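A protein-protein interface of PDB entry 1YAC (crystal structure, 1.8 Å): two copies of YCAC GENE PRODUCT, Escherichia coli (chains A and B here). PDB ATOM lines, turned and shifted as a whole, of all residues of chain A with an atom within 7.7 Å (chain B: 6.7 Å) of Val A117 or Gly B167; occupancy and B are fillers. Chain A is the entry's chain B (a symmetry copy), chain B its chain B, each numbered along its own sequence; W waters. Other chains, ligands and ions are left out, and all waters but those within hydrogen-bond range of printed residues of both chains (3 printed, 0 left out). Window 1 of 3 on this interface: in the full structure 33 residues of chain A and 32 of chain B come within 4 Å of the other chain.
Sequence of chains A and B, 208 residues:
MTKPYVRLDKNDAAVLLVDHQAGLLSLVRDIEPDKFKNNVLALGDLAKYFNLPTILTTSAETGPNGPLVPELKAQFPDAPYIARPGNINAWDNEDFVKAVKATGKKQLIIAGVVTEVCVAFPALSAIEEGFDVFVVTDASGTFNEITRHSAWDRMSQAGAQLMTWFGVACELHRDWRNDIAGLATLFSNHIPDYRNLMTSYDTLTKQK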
ATOM      1  N   VAL A  18       8.556 -14.439  11.334  1.00  0.00           N
ATOM      2  CA  VAL A  18       7.587 -13.772  10.489  1.00  0.00           C
ATOM      3  C   VAL A  18       8.025 -13.282   9.108  1.00  0.00           C
ATOM      4  O   VAL A  18       8.814 -12.343   8.984  1.00  0.00           O
ATOM      5  CB  VAL A  18       6.984 -12.552  11.260  1.00  0.00           C
ATOM      6  CG1 VAL A  18       5.769 -11.991  10.524  1.00  0.00           C
ATOM      7  CG2 VAL A  18       6.616 -12.951  12.688  1.00  0.00           C
ATOM      8  N   ASP A  19       7.480 -13.919   8.084  1.00  0.00           N
ATOM      9  CA  ASP A  19       7.689 -13.538   6.692  1.00  0.00           C
ATOM     10  C   ASP A  19       9.106 -13.544   6.094  1.00  0.00           C
ATOM     11  O   ASP A  19       9.443 -12.668   5.286  1.00  0.00           O
ATOM     12  CB  ASP A  19       7.007 -12.181   6.427  1.00  0.00           C
ATOM     13  CG  ASP A  19       5.525 -12.166   6.827  1.00  0.00           C
ATOM     14  OD1 ASP A  19       4.960 -13.228   7.147  1.00  0.00           O
ATOM     15  OD2 ASP A  19       4.925 -11.071   6.854  1.00  0.00           O
ATOM     16  N   ARG A  84      -0.878 -16.316   6.011  1.00  0.00           N
ATOM     17  CA  ARG A  84      -1.855 -15.245   6.129  1.00  0.00           C
ATOM     18  C   ARG A  84      -2.218 -14.749   4.741  1.00  0.00           C
ATOM     19  O   ARG A  84      -1.345 -14.353   3.960  1.00  0.00           O
ATOM     20  CB  ARG A  84      -1.283 -14.092   6.961  1.00  0.00           C
ATOM     21  CG  ARG A  84      -0.581 -14.554   8.228  1.00  0.00           C
ATOM     22  CD  ARG A  84      -0.342 -13.417   9.216  1.00  0.00           C
ATOM     23  NE  ARG A  84       0.340 -12.245   8.660  1.00  0.00           N
ATOM     24  CZ  ARG A  84       1.623 -12.190   8.306  1.00  0.00           C
ATOM     25  NH1 ARG A  84       2.418 -13.243   8.436  1.00  0.00           N
ATOM     26  NH2 ARG A  84       2.115 -11.075   7.794  1.00  0.00           N
ATOM     27  N   ILE A  88      -1.703  -7.943   7.476  1.00  0.00           N
ATOM     28  CA  ILE A  88      -0.320  -7.504   7.466  1.00  0.00           C
ATOM     29  C   ILE A  88       0.333  -7.756   8.828  1.00  0.00           C
ATOM     30  O   ILE A  88       1.417  -8.341   8.910  1.00  0.00           O
ATOM     31  CB  ILE A  88      -0.231  -6.049   7.008  1.00  0.00           C
ATOM     32  CG1 ILE A  88      -0.678  -5.966   5.540  1.00  0.00           C
ATOM     33  CG2 ILE A  88       1.192  -5.547   7.156  1.00  0.00           C
ATOM     34  CD1 ILE A  88      -0.804  -4.567   4.989  1.00  0.00           C
ATOM     35  N   ASN A  89      -0.316  -7.300   9.897  1.00  0.00           N
ATOM     36  CA  ASN A  89       0.180  -7.548  11.257  1.00  0.00           C
ATOM     37  C   ASN A  89      -0.291  -8.978  11.575  1.00  0.00           C
ATOM     38  O   ASN A  89      -1.503  -9.267  11.597  1.00  0.00           O
ATOM     39  CB  ASN A  89      -0.442  -6.563  12.246  1.00  0.00           C
ATOM     40  CG  ASN A  89      -0.054  -6.851  13.683  1.00  0.00           C
ATOM     41  OD1 ASN A  89       0.706  -7.771  13.983  1.00  0.00           O
ATOM     42  ND2 ASN A  89      -0.583  -6.053  14.590  1.00  0.00           N
ATOM     43  N   ALA A  90       0.663  -9.891  11.770  1.00  0.00           N
ATOM     44  CA  ALA A  90       0.344 -11.287  12.083  1.00  0.00           C
ATOM     45  C   ALA A  90      -0.580 -11.435  13.291  1.00  0.00           C
ATOM     46  O   ALA A  90      -1.343 -12.391  13.368  1.00  0.00           O
ATOM     47  CB  ALA A  90       1.625 -12.092  12.300  1.00  0.00           C
ATOM     48  N   GLY A 112      11.876 -11.189  11.652  1.00  0.00           N
ATOM     49  CA  GLY A 112      11.143 -11.256  10.402  1.00  0.00           C
ATOM     50  C   GLY A 112      11.483 -10.136   9.447  1.00  0.00           C
ATOM     51  O   GLY A 112      12.448  -9.405   9.662  1.00  0.00           O
ATOM     52  N   VAL A 113      10.723 -10.033   8.360  1.00  0.00           N
ATOM     53  CA  VAL A 113      10.958  -8.977   7.387  1.00  0.00           C
ATOM     54  C   VAL A 113       9.635  -8.455   6.883  1.00  0.00           C
ATOM     55  O   VAL A 113       8.700  -9.239   6.668  1.00  0.00           O
ATOM     56  CB  VAL A 113      11.850  -9.429   6.173  1.00  0.00           C
ATOM     57  CG1 VAL A 113      12.926 -10.419   6.587  1.00  0.00           C
ATOM     58  CG2 VAL A 113      11.045  -9.980   5.092  1.00  0.00           C
ATOM     59  N   VAL A 114       9.454  -7.139   6.781  1.00  0.00           N
ATOM     60  CA  VAL A 114      10.419  -6.089   7.116  1.00  0.00           C
ATOM     61  C   VAL A 114      10.276  -5.760   8.600  1.00  0.00           C
ATOM     62  O   VAL A 114       9.189  -5.834   9.179  1.00  0.00           O
ATOM     63  CB  VAL A 114      10.286  -4.810   6.241  1.00  0.00           C
ATOM     64  CG1 VAL A 114      10.467  -5.183   4.753  1.00  0.00           C
ATOM     65  CG2 VAL A 114       8.952  -4.095   6.498  1.00  0.00           C
ATOM     66  N   THR A 115      11.384  -5.396   9.215  1.00  0.00           N
ATOM     67  CA  THR A 115      11.395  -5.123  10.644  1.00  0.00           C
ATOM     68  C   THR A 115      10.369  -4.120  11.199  1.00  0.00           C
ATOM     69  O   THR A 115       9.789  -4.360  12.263  1.00  0.00           O
ATOM     70  CB  THR A 115      12.814  -4.739  11.099  1.00  0.00           C
ATOM     71  OG1 THR A 115      13.107  -3.430  10.678  1.00  0.00           O
ATOM     72  CG2 THR A 115      13.809  -5.607  10.424  1.00  0.00           C
ATOM     73  N   GLU A 116      10.061  -3.068  10.442  1.00  0.00           N
ATOM     74  CA  GLU A 116       9.135  -2.040  10.919  1.00  0.00           C
ATOM     75  C   GLU A 116       7.663  -2.409  10.750  1.00  0.00           C
ATOM     76  O   GLU A 116       6.778  -1.711  11.244  1.00  0.00           O
ATOM     77  CB  GLU A 116       9.428  -0.683  10.252  1.00  0.00           C
ATOM     78  CG  GLU A 116       8.973  -0.539   8.791  1.00  0.00           C
ATOM     79  CD  GLU A 116      10.005  -0.997   7.769  1.00  0.00           C
ATOM     80  OE1 GLU A 116      10.840  -1.870   8.108  1.00  0.00           O
ATOM     81  OE2 GLU A 116       9.970  -0.480   6.623  1.00  0.00           O
ATOM     82  N   VAL A 117       7.405  -3.509  10.047  1.00  0.00           N
ATOM     83  CA  VAL A 117       6.039  -3.946   9.818  1.00  0.00           C
ATOM     84  C   VAL A 117       5.811  -5.342  10.377  1.00  0.00           C
ATOM     85  O   VAL A 117       5.160  -5.500  11.412  1.00  0.00           O
ATOM     86  CB  VAL A 117       5.661  -3.935   8.299  1.00  0.00           C
ATOM     87  CG1 VAL A 117       4.285  -4.597   8.081  1.00  0.00           C
ATOM     88  CG2 VAL A 117       5.621  -2.527   7.765  1.00  0.00           C
ATOM     89  N   CYS A 118       6.382  -6.349   9.724  1.00  0.00           N
ATOM     90  CA  CYS A 118       6.161  -7.720  10.156  1.00  0.00           C
ATOM     91  C   CYS A 118       6.707  -8.095  11.510  1.00  0.00           C
ATOM     92  O   CYS A 118       6.273  -9.091  12.082  1.00  0.00           O
ATOM     93  CB  CYS A 118       6.575  -8.707   9.082  1.00  0.00           C
ATOM     94  SG  CYS A 118       5.704  -8.360   7.552  1.00  0.00           S
ATOM     95  N   VAL A 119       7.670  -7.331  12.016  1.00  0.00           N
ATOM     96  CA  VAL A 119       8.200  -7.592  13.351  1.00  0.00           C
ATOM     97  C   VAL A 119       7.566  -6.599  14.324  1.00  0.00           C
ATOM     98  O   VAL A 119       6.911  -6.989  15.298  1.00  0.00           O
ATOM     99  CB  VAL A 119       9.744  -7.456  13.398  1.00  0.00           C
ATOM    100  CG1 VAL A 119      10.248  -7.512  14.836  1.00  0.00           C
ATOM    101  CG2 VAL A 119      10.377  -8.574  12.585  1.00  0.00           C
ATOM    102  N   ALA A 120       7.724  -5.312  14.037  1.00  0.00           N
ATOM    103  CA  ALA A 120       7.198  -4.265  14.917  1.00  0.00           C
ATOM    104  C   ALA A 120       5.710  -4.353  15.257  1.00  0.00           C
ATOM    105  O   ALA A 120       5.334  -4.205  16.424  1.00  0.00           O
ATOM    106  CB  ALA A 120       7.524  -2.883  14.355  1.00  0.00           C
ATOM    107  N   PHE A 121       4.870  -4.617  14.261  1.00  0.00           N
ATOM    108  CA  PHE A 121       3.426  -4.660  14.514  1.00  0.00           C
ATOM    109  C   PHE A 121       3.073  -5.757  15.511  1.00  0.00           C
ATOM    110  O   PHE A 121       2.463  -5.469  16.544  1.00  0.00           O
ATOM    111  CB  PHE A 121       2.608  -4.777  13.215  1.00  0.00           C
ATOM    112  CG  PHE A 121       2.700  -3.562  12.312  1.00  0.00           C
ATOM    113  CD1 PHE A 121       3.558  -2.500  12.610  1.00  0.00           C
ATOM    114  CD2 PHE A 121       1.959  -3.506  11.130  1.00  0.00           C
ATOM    115  CE1 PHE A 121       3.681  -1.410  11.742  1.00  0.00           C
ATOM    116  CE2 PHE A 121       2.077  -2.412  10.255  1.00  0.00           C
ATOM    117  CZ  PHE A 121       2.939  -1.368  10.564  1.00  0.00           C
ATOM    118  N   PRO A 122       3.468  -7.017  15.237  1.00  0.00           N
ATOM    119  CA  PRO A 122       3.113  -8.039  16.226  1.00  0.00           C
ATOM    120  C   PRO A 122       3.826  -7.850  17.569  1.00  0.00           C
ATOM    121  O   PRO A 122       3.260  -8.173  18.616  1.00  0.00           O
ATOM    122  CB  PRO A 122       3.459  -9.358  15.518  1.00  0.00           C
ATOM    123  CG  PRO A 122       4.449  -8.967  14.460  1.00  0.00           C
ATOM    124  CD  PRO A 122       3.951  -7.638  13.989  1.00  0.00           C
ATOM    125  N   ALA A 123       5.043  -7.303  17.559  1.00  0.00           N
ATOM    126  CA  ALA A 123       5.755  -7.064  18.819  1.00  0.00           C
ATOM    127  C   ALA A 123       4.946  -6.077  19.678  1.00  0.00           C
ATOM    128  O   ALA A 123       4.711  -6.314  20.869  1.00  0.00           O
ATOM    129  CB  ALA A 123       7.157  -6.503  18.561  1.00  0.00           C
ATOM    130  N   LEU A 124       4.489  -4.991  19.062  1.00  0.00           N
ATOM    131  CA  LEU A 124       3.720  -3.974  19.783  1.00  0.00           C
ATOM    132  C   LEU A 124       2.391  -4.543  20.278  1.00  0.00           C
ATOM    133  O   LEU A 124       1.952  -4.232  21.390  1.00  0.00           O
ATOM    134  CB  LEU A 124       3.491  -2.739  18.902  1.00  0.00           C
ATOM    135  CG  LEU A 124       4.783  -1.994  18.527  1.00  0.00           C
ATOM    136  CD1 LEU A 124       4.515  -0.919  17.471  1.00  0.00           C
ATOM    137  CD2 LEU A 124       5.408  -1.386  19.759  1.00  0.00           C
ATOM    138  N   GLY A 141      15.109  -7.925   8.848  1.00  0.00           N
ATOM    139  CA  GLY A 141      15.627  -7.066   7.791  1.00  0.00           C
ATOM    140  C   GLY A 141      14.661  -6.039   7.241  1.00  0.00           C
ATOM    141  O   GLY A 141      13.449  -6.245   7.252  1.00  0.00           O
ATOM    142  N   THR A 142      15.196  -4.945   6.713  1.00  0.00           N
ATOM    143  CA  THR A 142      14.351  -3.894   6.159  1.00  0.00           C
ATOM    144  C   THR A 142      15.048  -3.108   5.035  1.00  0.00           C
ATOM    145  O   THR A 142      16.146  -3.473   4.604  1.00  0.00           O
ATOM    146  CB  THR A 142      13.823  -2.957   7.299  1.00  0.00           C
ATOM    147  OG1 THR A 142      12.938  -1.977   6.750  1.00  0.00           O
ATOM    148  CG2 THR A 142      14.974  -2.238   8.010  1.00  0.00           C
ATOM    149  N   PHE A 143      14.412  -2.035   4.576  1.00  0.00           N
ATOM    150  CA  PHE A 143      14.932  -1.210   3.479  1.00  0.00           C
ATOM    151  C   PHE A 143      16.280  -0.537   3.708  1.00  0.00           C
ATOM    152  O   PHE A 143      17.175  -0.621   2.864  1.00  0.00           O
ATOM    153  CB  PHE A 143      13.903  -0.138   3.087  1.00  0.00           C
ATOM    154  CG  PHE A 143      12.548  -0.693   2.773  1.00  0.00           C
ATOM    155  CD1 PHE A 143      12.272  -1.214   1.508  1.00  0.00           C
ATOM    156  CD2 PHE A 143      11.551  -0.718   3.747  1.00  0.00           C
ATOM    157  CE1 PHE A 143      11.025  -1.753   1.213  1.00  0.00           C
ATOM    158  CE2 PHE A 143      10.299  -1.256   3.473  1.00  0.00           C
ATOM    159  CZ  PHE A 143      10.029  -1.778   2.200  1.00  0.00           C
ATOM    160  N   THR A 147      14.613   3.137   8.198  1.00  0.00           N
ATOM    161  CA  THR A 147      13.439   2.318   8.483  1.00  0.00           C
ATOM    162  C   THR A 147      13.733   1.379   9.662  1.00  0.00           C
ATOM    163  O   THR A 147      12.861   1.122  10.503  1.00  0.00           O
ATOM    164  CB  THR A 147      12.965   1.535   7.233  1.00  0.00           C
ATOM    165  OG1 THR A 147      14.021   0.682   6.750  1.00  0.00           O
ATOM    166  CG2 THR A 147      12.578   2.508   6.132  1.00  0.00           C
ATOM    167  N   ALA A 151      12.149   1.868  13.670  1.00  0.00           N
ATOM    168  CA  ALA A 151      11.434   0.728  14.250  1.00  0.00           C
ATOM    169  C   ALA A 151      12.010   0.362  15.610  1.00  0.00           C
ATOM    170  O   ALA A 151      11.264   0.066  16.529  1.00  0.00           O
ATOM    171  CB  ALA A 151      11.481  -0.468  13.315  1.00  0.00           C
ATOM    172  N   ARG A 154      10.705   2.762  18.101  1.00  0.00           N
ATOM    173  CA  ARG A 154       9.303   2.482  18.375  1.00  0.00           C
ATOM    174  C   ARG A 154       9.120   1.245  19.262  1.00  0.00           C
ATOM    175  O   ARG A 154       8.364   1.272  20.234  1.00  0.00           O
ATOM    176  CB  ARG A 154       8.525   2.320  17.062  1.00  0.00           C
ATOM    177  CG  ARG A 154       7.012   2.514  17.241  1.00  0.00           C
ATOM    178  CD  ARG A 154       6.215   2.288  15.961  1.00  0.00           C
ATOM    179  NE  ARG A 154       4.795   2.599  16.158  1.00  0.00           N
ATOM    180  CZ  ARG A 154       3.816   2.144  15.388  1.00  0.00           C
ATOM    181  NH1 ARG A 154       4.085   1.346  14.364  1.00  0.00           N
ATOM    182  NH2 ARG A 154       2.565   2.513  15.626  1.00  0.00           N
ATOM    183  N   MET A 155       9.834   0.170  18.945  1.00  0.00           N
ATOM    184  CA  MET A 155       9.735  -1.055  19.720  1.00  0.00           C
ATOM    185  C   MET A 155      10.296  -0.900  21.138  1.00  0.00           C
ATOM    186  O   MET A 155       9.677  -1.342  22.118  1.00  0.00           O
ATOM    187  CB  MET A 155      10.408  -2.210  18.975  1.00  0.00           C
ATOM    188  CG  MET A 155       9.667  -2.593  17.686  1.00  0.00           C
ATOM    189  SD  MET A 155      10.343  -4.030  16.853  1.00  0.00           S
ATOM    190  CE  MET A 155      11.882  -3.384  16.229  1.00  0.00           C
ATOM    191  N   TYR B   5      -0.686  -0.476  22.166  1.00  0.00           N
ATOM    192  CA  TYR B   5      -0.159  -0.301  20.824  1.00  0.00           C
ATOM    193  C   TYR B   5      -1.055   0.763  20.187  1.00  0.00           C
ATOM    194  O   TYR B   5      -2.190   0.485  19.794  1.00  0.00           O
ATOM    195  CB  TYR B   5      -0.245  -1.645  20.091  1.00  0.00           C
ATOM    196  CG  TYR B   5       0.139  -1.682  18.627  1.00  0.00           C
ATOM    197  CD1 TYR B   5       0.820  -0.632  18.007  1.00  0.00           C
ATOM    198  CD2 TYR B   5      -0.202  -2.785  17.858  1.00  0.00           C
ATOM    199  CE1 TYR B   5       1.138  -0.692  16.646  1.00  0.00           C
ATOM    200  CE2 TYR B   5       0.103  -2.859  16.519  1.00  0.00           C
ATOM    201  CZ  TYR B   5       0.765  -1.815  15.909  1.00  0.00           C
ATOM    202  OH  TYR B   5       0.984  -1.903  14.549  1.00  0.00           O
ATOM    203  N   LEU B   8      -1.976   3.414  13.879  1.00  0.00           N
ATOM    204  CA  LEU B   8      -2.652   4.251  12.904  1.00  0.00           C
ATOM    205  C   LEU B   8      -3.977   3.653  12.510  1.00  0.00           C
ATOM    206  O   LEU B   8      -4.077   2.454  12.251  1.00  0.00           O
ATOM    207  CB  LEU B   8      -1.784   4.471  11.667  1.00  0.00           C
ATOM    208  CG  LEU B   8      -0.585   5.409  11.869  1.00  0.00           C
ATOM    209  CD1 LEU B   8       0.296   5.441  10.612  1.00  0.00           C
ATOM    210  CD2 LEU B   8      -1.086   6.801  12.191  1.00  0.00           C
ATOM    211  N   MET B 163       8.025   6.554  12.618  1.00  0.00           N
ATOM    212  CA  MET B 163       7.640   5.608  11.579  1.00  0.00           C
ATOM    213  C   MET B 163       8.222   6.008  10.219  1.00  0.00           C
ATOM    214  O   MET B 163       8.887   7.038  10.090  1.00  0.00           O
ATOM    215  CB  MET B 163       6.108   5.469  11.509  1.00  0.00           C
ATOM    216  CG  MET B 163       5.512   4.651  12.691  1.00  0.00           C
ATOM    217  SD  MET B 163       3.766   4.410  12.502  1.00  0.00           S
ATOM    218  CE  MET B 163       3.738   3.015  11.416  1.00  0.00           C
ATOM    219  N   THR B 164       8.057   5.135   9.232  1.00  0.00           N
ATOM    220  CA  THR B 164       8.561   5.395   7.893  1.00  0.00           C
ATOM    221  C   THR B 164       7.397   5.126   6.954  1.00  0.00           C
ATOM    222  O   THR B 164       6.484   4.363   7.314  1.00  0.00           O
ATOM    223  CB  THR B 164       9.877   4.597   7.607  1.00  0.00           C
ATOM    224  OG1 THR B 164       9.791   3.260   8.128  1.00  0.00           O
ATOM    225  CG2 THR B 164      11.050   5.304   8.297  1.00  0.00           C
ATOM    226  N   TRP B 165       7.408   5.722   5.761  1.00  0.00           N
ATOM    227  CA  TRP B 165       6.245   5.618   4.875  1.00  0.00           C
ATOM    228  C   TRP B 165       5.646   4.255   4.590  1.00  0.00           C
ATOM    229  O   TRP B 165       4.431   4.111   4.641  1.00  0.00           O
ATOM    230  CB  TRP B 165       6.410   6.464   3.594  1.00  0.00           C
ATOM    231  CG  TRP B 165       7.158   5.795   2.467  1.00  0.00           C
ATOM    232  CD1 TRP B 165       8.463   5.988   2.120  1.00  0.00           C
ATOM    233  CD2 TRP B 165       6.651   4.793   1.580  1.00  0.00           C
ATOM    234  NE1 TRP B 165       8.805   5.157   1.086  1.00  0.00           N
ATOM    235  CE2 TRP B 165       7.713   4.411   0.736  1.00  0.00           C
ATOM    236  CE3 TRP B 165       5.400   4.173   1.426  1.00  0.00           C
ATOM    237  CZ2 TRP B 165       7.571   3.435  -0.252  1.00  0.00           C
ATOM    238  CZ3 TRP B 165       5.259   3.194   0.434  1.00  0.00           C
ATOM    239  CH2 TRP B 165       6.340   2.838  -0.387  1.00  0.00           C
ATOM    240  N   PHE B 166       6.470   3.245   4.332  1.00  0.00           N
ATOM    241  CA  PHE B 166       5.944   1.901   4.054  1.00  0.00           C
ATOM    242  C   PHE B 166       5.229   1.351   5.294  1.00  0.00           C
ATOM    243  O   PHE B 166       4.151   0.765   5.188  1.00  0.00           O
ATOM    244  CB  PHE B 166       7.074   0.965   3.601  1.00  0.00           C
ATOM    245  CG  PHE B 166       6.633  -0.449   3.326  1.00  0.00           C
ATOM    246  CD1 PHE B 166       6.012  -0.779   2.120  1.00  0.00           C
ATOM    247  CD2 PHE B 166       6.882  -1.463   4.251  1.00  0.00           C
ATOM    248  CE1 PHE B 166       5.650  -2.105   1.840  1.00  0.00           C
ATOM    249  CE2 PHE B 166       6.524  -2.790   3.982  1.00  0.00           C
ATOM    250  CZ  PHE B 166       5.908  -3.110   2.774  1.00  0.00           C
ATOM    251  N   GLY B 167       5.825   1.569   6.466  1.00  0.00           N
ATOM    252  CA  GLY B 167       5.219   1.120   7.708  1.00  0.00           C
ATOM    253  C   GLY B 167       3.895   1.842   7.910  1.00  0.00           C
ATOM    254  O   GLY B 167       2.916   1.236   8.325  1.00  0.00           O
ATOM    255  N   VAL B 168       3.869   3.137   7.608  1.00  0.00           N
ATOM    256  CA  VAL B 168       2.655   3.953   7.731  1.00  0.00           C
ATOM    257  C   VAL B 168       1.555   3.345   6.850  1.00  0.00           C
ATOM    258  O   VAL B 168       0.439   3.107   7.317  1.00  0.00           O
ATOM    259  CB  VAL B 168       2.921   5.452   7.318  1.00  0.00           C
ATOM    260  CG1 VAL B 168       1.608   6.235   7.168  1.00  0.00           C
ATOM    261  CG2 VAL B 168       3.805   6.133   8.359  1.00  0.00           C
ATOM    262  N   ALA B 169       1.894   3.036   5.601  1.00  0.00           N
ATOM    263  CA  ALA B 169       0.936   2.449   4.670  1.00  0.00           C
ATOM    264  C   ALA B 169       0.390   1.110   5.164  1.00  0.00           C
ATOM    265  O   ALA B 169      -0.824   0.870   5.101  1.00  0.00           O
ATOM    266  CB  ALA B 169       1.570   2.272   3.304  1.00  0.00           C
ATOM    267  N   CYS B 170       1.273   0.251   5.670  1.00  0.00           N
ATOM    268  CA  CYS B 170       0.860  -1.070   6.159  1.00  0.00           C
ATOM    269  C   CYS B 170       0.015  -1.003   7.431  1.00  0.00           C
ATOM    270  O   CYS B 170      -0.913  -1.799   7.606  1.00  0.00           O
ATOM    271  CB  CYS B 170       2.075  -1.971   6.401  1.00  0.00           C
ATOM    272  SG  CYS B 170       2.954  -2.441   4.906  1.00  0.00           S
ATOM    273  N   GLU B 171       0.327  -0.058   8.317  1.00  0.00           N
ATOM    274  CA  GLU B 171      -0.421   0.066   9.553  1.00  0.00           C
ATOM    275  C   GLU B 171      -1.811   0.606   9.263  1.00  0.00           C
ATOM    276  O   GLU B 171      -2.777   0.203   9.896  1.00  0.00           O
ATOM    277  CB  GLU B 171       0.319   0.936  10.569  1.00  0.00           C
ATOM    278  CG  GLU B 171      -0.240   0.779  11.999  1.00  0.00           C
ATOM    279  CD  GLU B 171       0.724   1.230  13.064  1.00  0.00           C
ATOM    280  OE1 GLU B 171       1.594   0.438  13.439  1.00  0.00           O
ATOM    281  OE2 GLU B 171       0.611   2.370  13.541  1.00  0.00           O
ATOM    282  N   LEU B 172      -1.911   1.502   8.287  1.00  0.00           N
ATOM    283  CA  LEU B 172      -3.203   2.062   7.907  1.00  0.00           C
ATOM    284  C   LEU B 172      -4.065   1.029   7.180  1.00  0.00           C
ATOM    285  O   LEU B 172      -5.262   0.919   7.451  1.00  0.00           O
ATOM    286  CB  LEU B 172      -3.009   3.271   6.987  1.00  0.00           C
ATOM    287  CG  LEU B 172      -2.517   4.589   7.594  1.00  0.00           C
ATOM    288  CD1 LEU B 172      -2.003   5.493   6.497  1.00  0.00           C
ATOM    289  CD2 LEU B 172      -3.654   5.273   8.346  1.00  0.00           C
HETATM  290  O   HOH W   1      10.357   2.426  10.560  1.00  0.00           O
HETATM  291  O   HOH W   2       8.755   1.842   6.199  1.00  0.00           O
HETATM  292  O   HOH W   3      -0.873  -3.267  12.872  1.00  0.00           O
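The guanidinium group (NH1) of Arg A154 lies close to the side-chain sulfur (SD) of Met B163 (3.6 Å). NH1 of Arg A154 is in salt-bridge range of OE1 of Glu B171.
The side-chain carboxylate (OE1) of Glu B171 is in hydrogen-bond range of the side-chain hydroxyl (OH) of Tyr B5 (2.7 Å). N of Leu B8 is in hydrogen-bond range of OE2 of Glu B171. O of Phe B166 is in hydrogen-bond range of SG of Cys B170, 3.4 Å away. NH2 of Arg A84 lies within hydrogen-bond range of O of Ile A88, at 3.0 Å. OE1 of Glu A116 lies within hydrogen-bond range of OG1 of Thr A142, 2.5 Å away. The side-chain hydroxyl of Thr A142 lies within hydrogen-bond range of the side-chain hydroxyl of Thr A147, at 2.9 Å.
Tyr B5 touches Asn A89 (CE2 to ND2, 3.8 Å). CE2 of Phe B166 touches CG2 of Val A114 (3.7 Å). Glu A116 touches Thr B164. Gly B167 touches Val A117 (CA to CG2, 3.7 Å). Gly B167 touches Phe A121 (O to CZ, 3.4 Å). CE1 of Phe A121 touches OE1 of Glu B171, 3.3 Å away. CE1 of Tyr B5 touches CD1 of Leu A124 (3.5 Å). Phe A143 touches Phe B166 (CE2 to CD2, 3.5 Å). Thr B164 touches Thr A147 (OG1 to CG2, 3.5 Å). CE1 of Tyr B5 touches NH2 of Arg A154 (3.7 Å).
Of the printed residues of chain B, Val A114 touches Phe B166 (3.7 Å). Of chain B, only Phe B166 (3.9 Å), Gly B167 (3.7 Å) and Cys B170 (3.8 Å) come within 4 Å of Val A117. Of the printed residues of chain A, Met B163 touches Arg A154 (3.4 Å). Printed residues of chain A within 4 Å of Phe B166: Val A114 (3.7 Å), Val A117 (3.9 Å) and Phe A143 (3.5 Å). Printed residues of chain A within 4 Å of Gly B167: Val A117 (3.7 Å) and Phe A121 (3.4 Å). The nearest printed residue of chain B that does not touch Thr A147 is Trp B165 (6.1 Å).
Of the 12 printed residues of chain B, 7 touch a printed residue of chain A. Along chain A the printed residues that touch a printed residue of chain B span positions 88 to 154. Among the printed residues, 17 pairs touch across the chains.
No position is printed for both chains. Of the 17 pairs that touch across the chains among the printed residues, none has its exchanged pair printed and touching as well.
Water W2 lies within hydrogen-bond range of the side-chain hydroxyl (OG1) of Thr B164 (2.6 Å), the side-chain carboxylate (OE2) of Glu A116 (2.7 Å), the backbone NH (N) of Gly B167 (3.0 Å) and the backbone NH (N) of Phe B166 (3.3 Å). Water W1 bridges the side-chain hydroxyl of Thr B164 (2.6 Å) and the backbone carbonyl oxygen of Thr A147 (2.8 Å). Water W3 lies within hydrogen-bond range of OH of Tyr B5 (2.8 Å) and ND2 of Asn A89 (3.3 Å).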
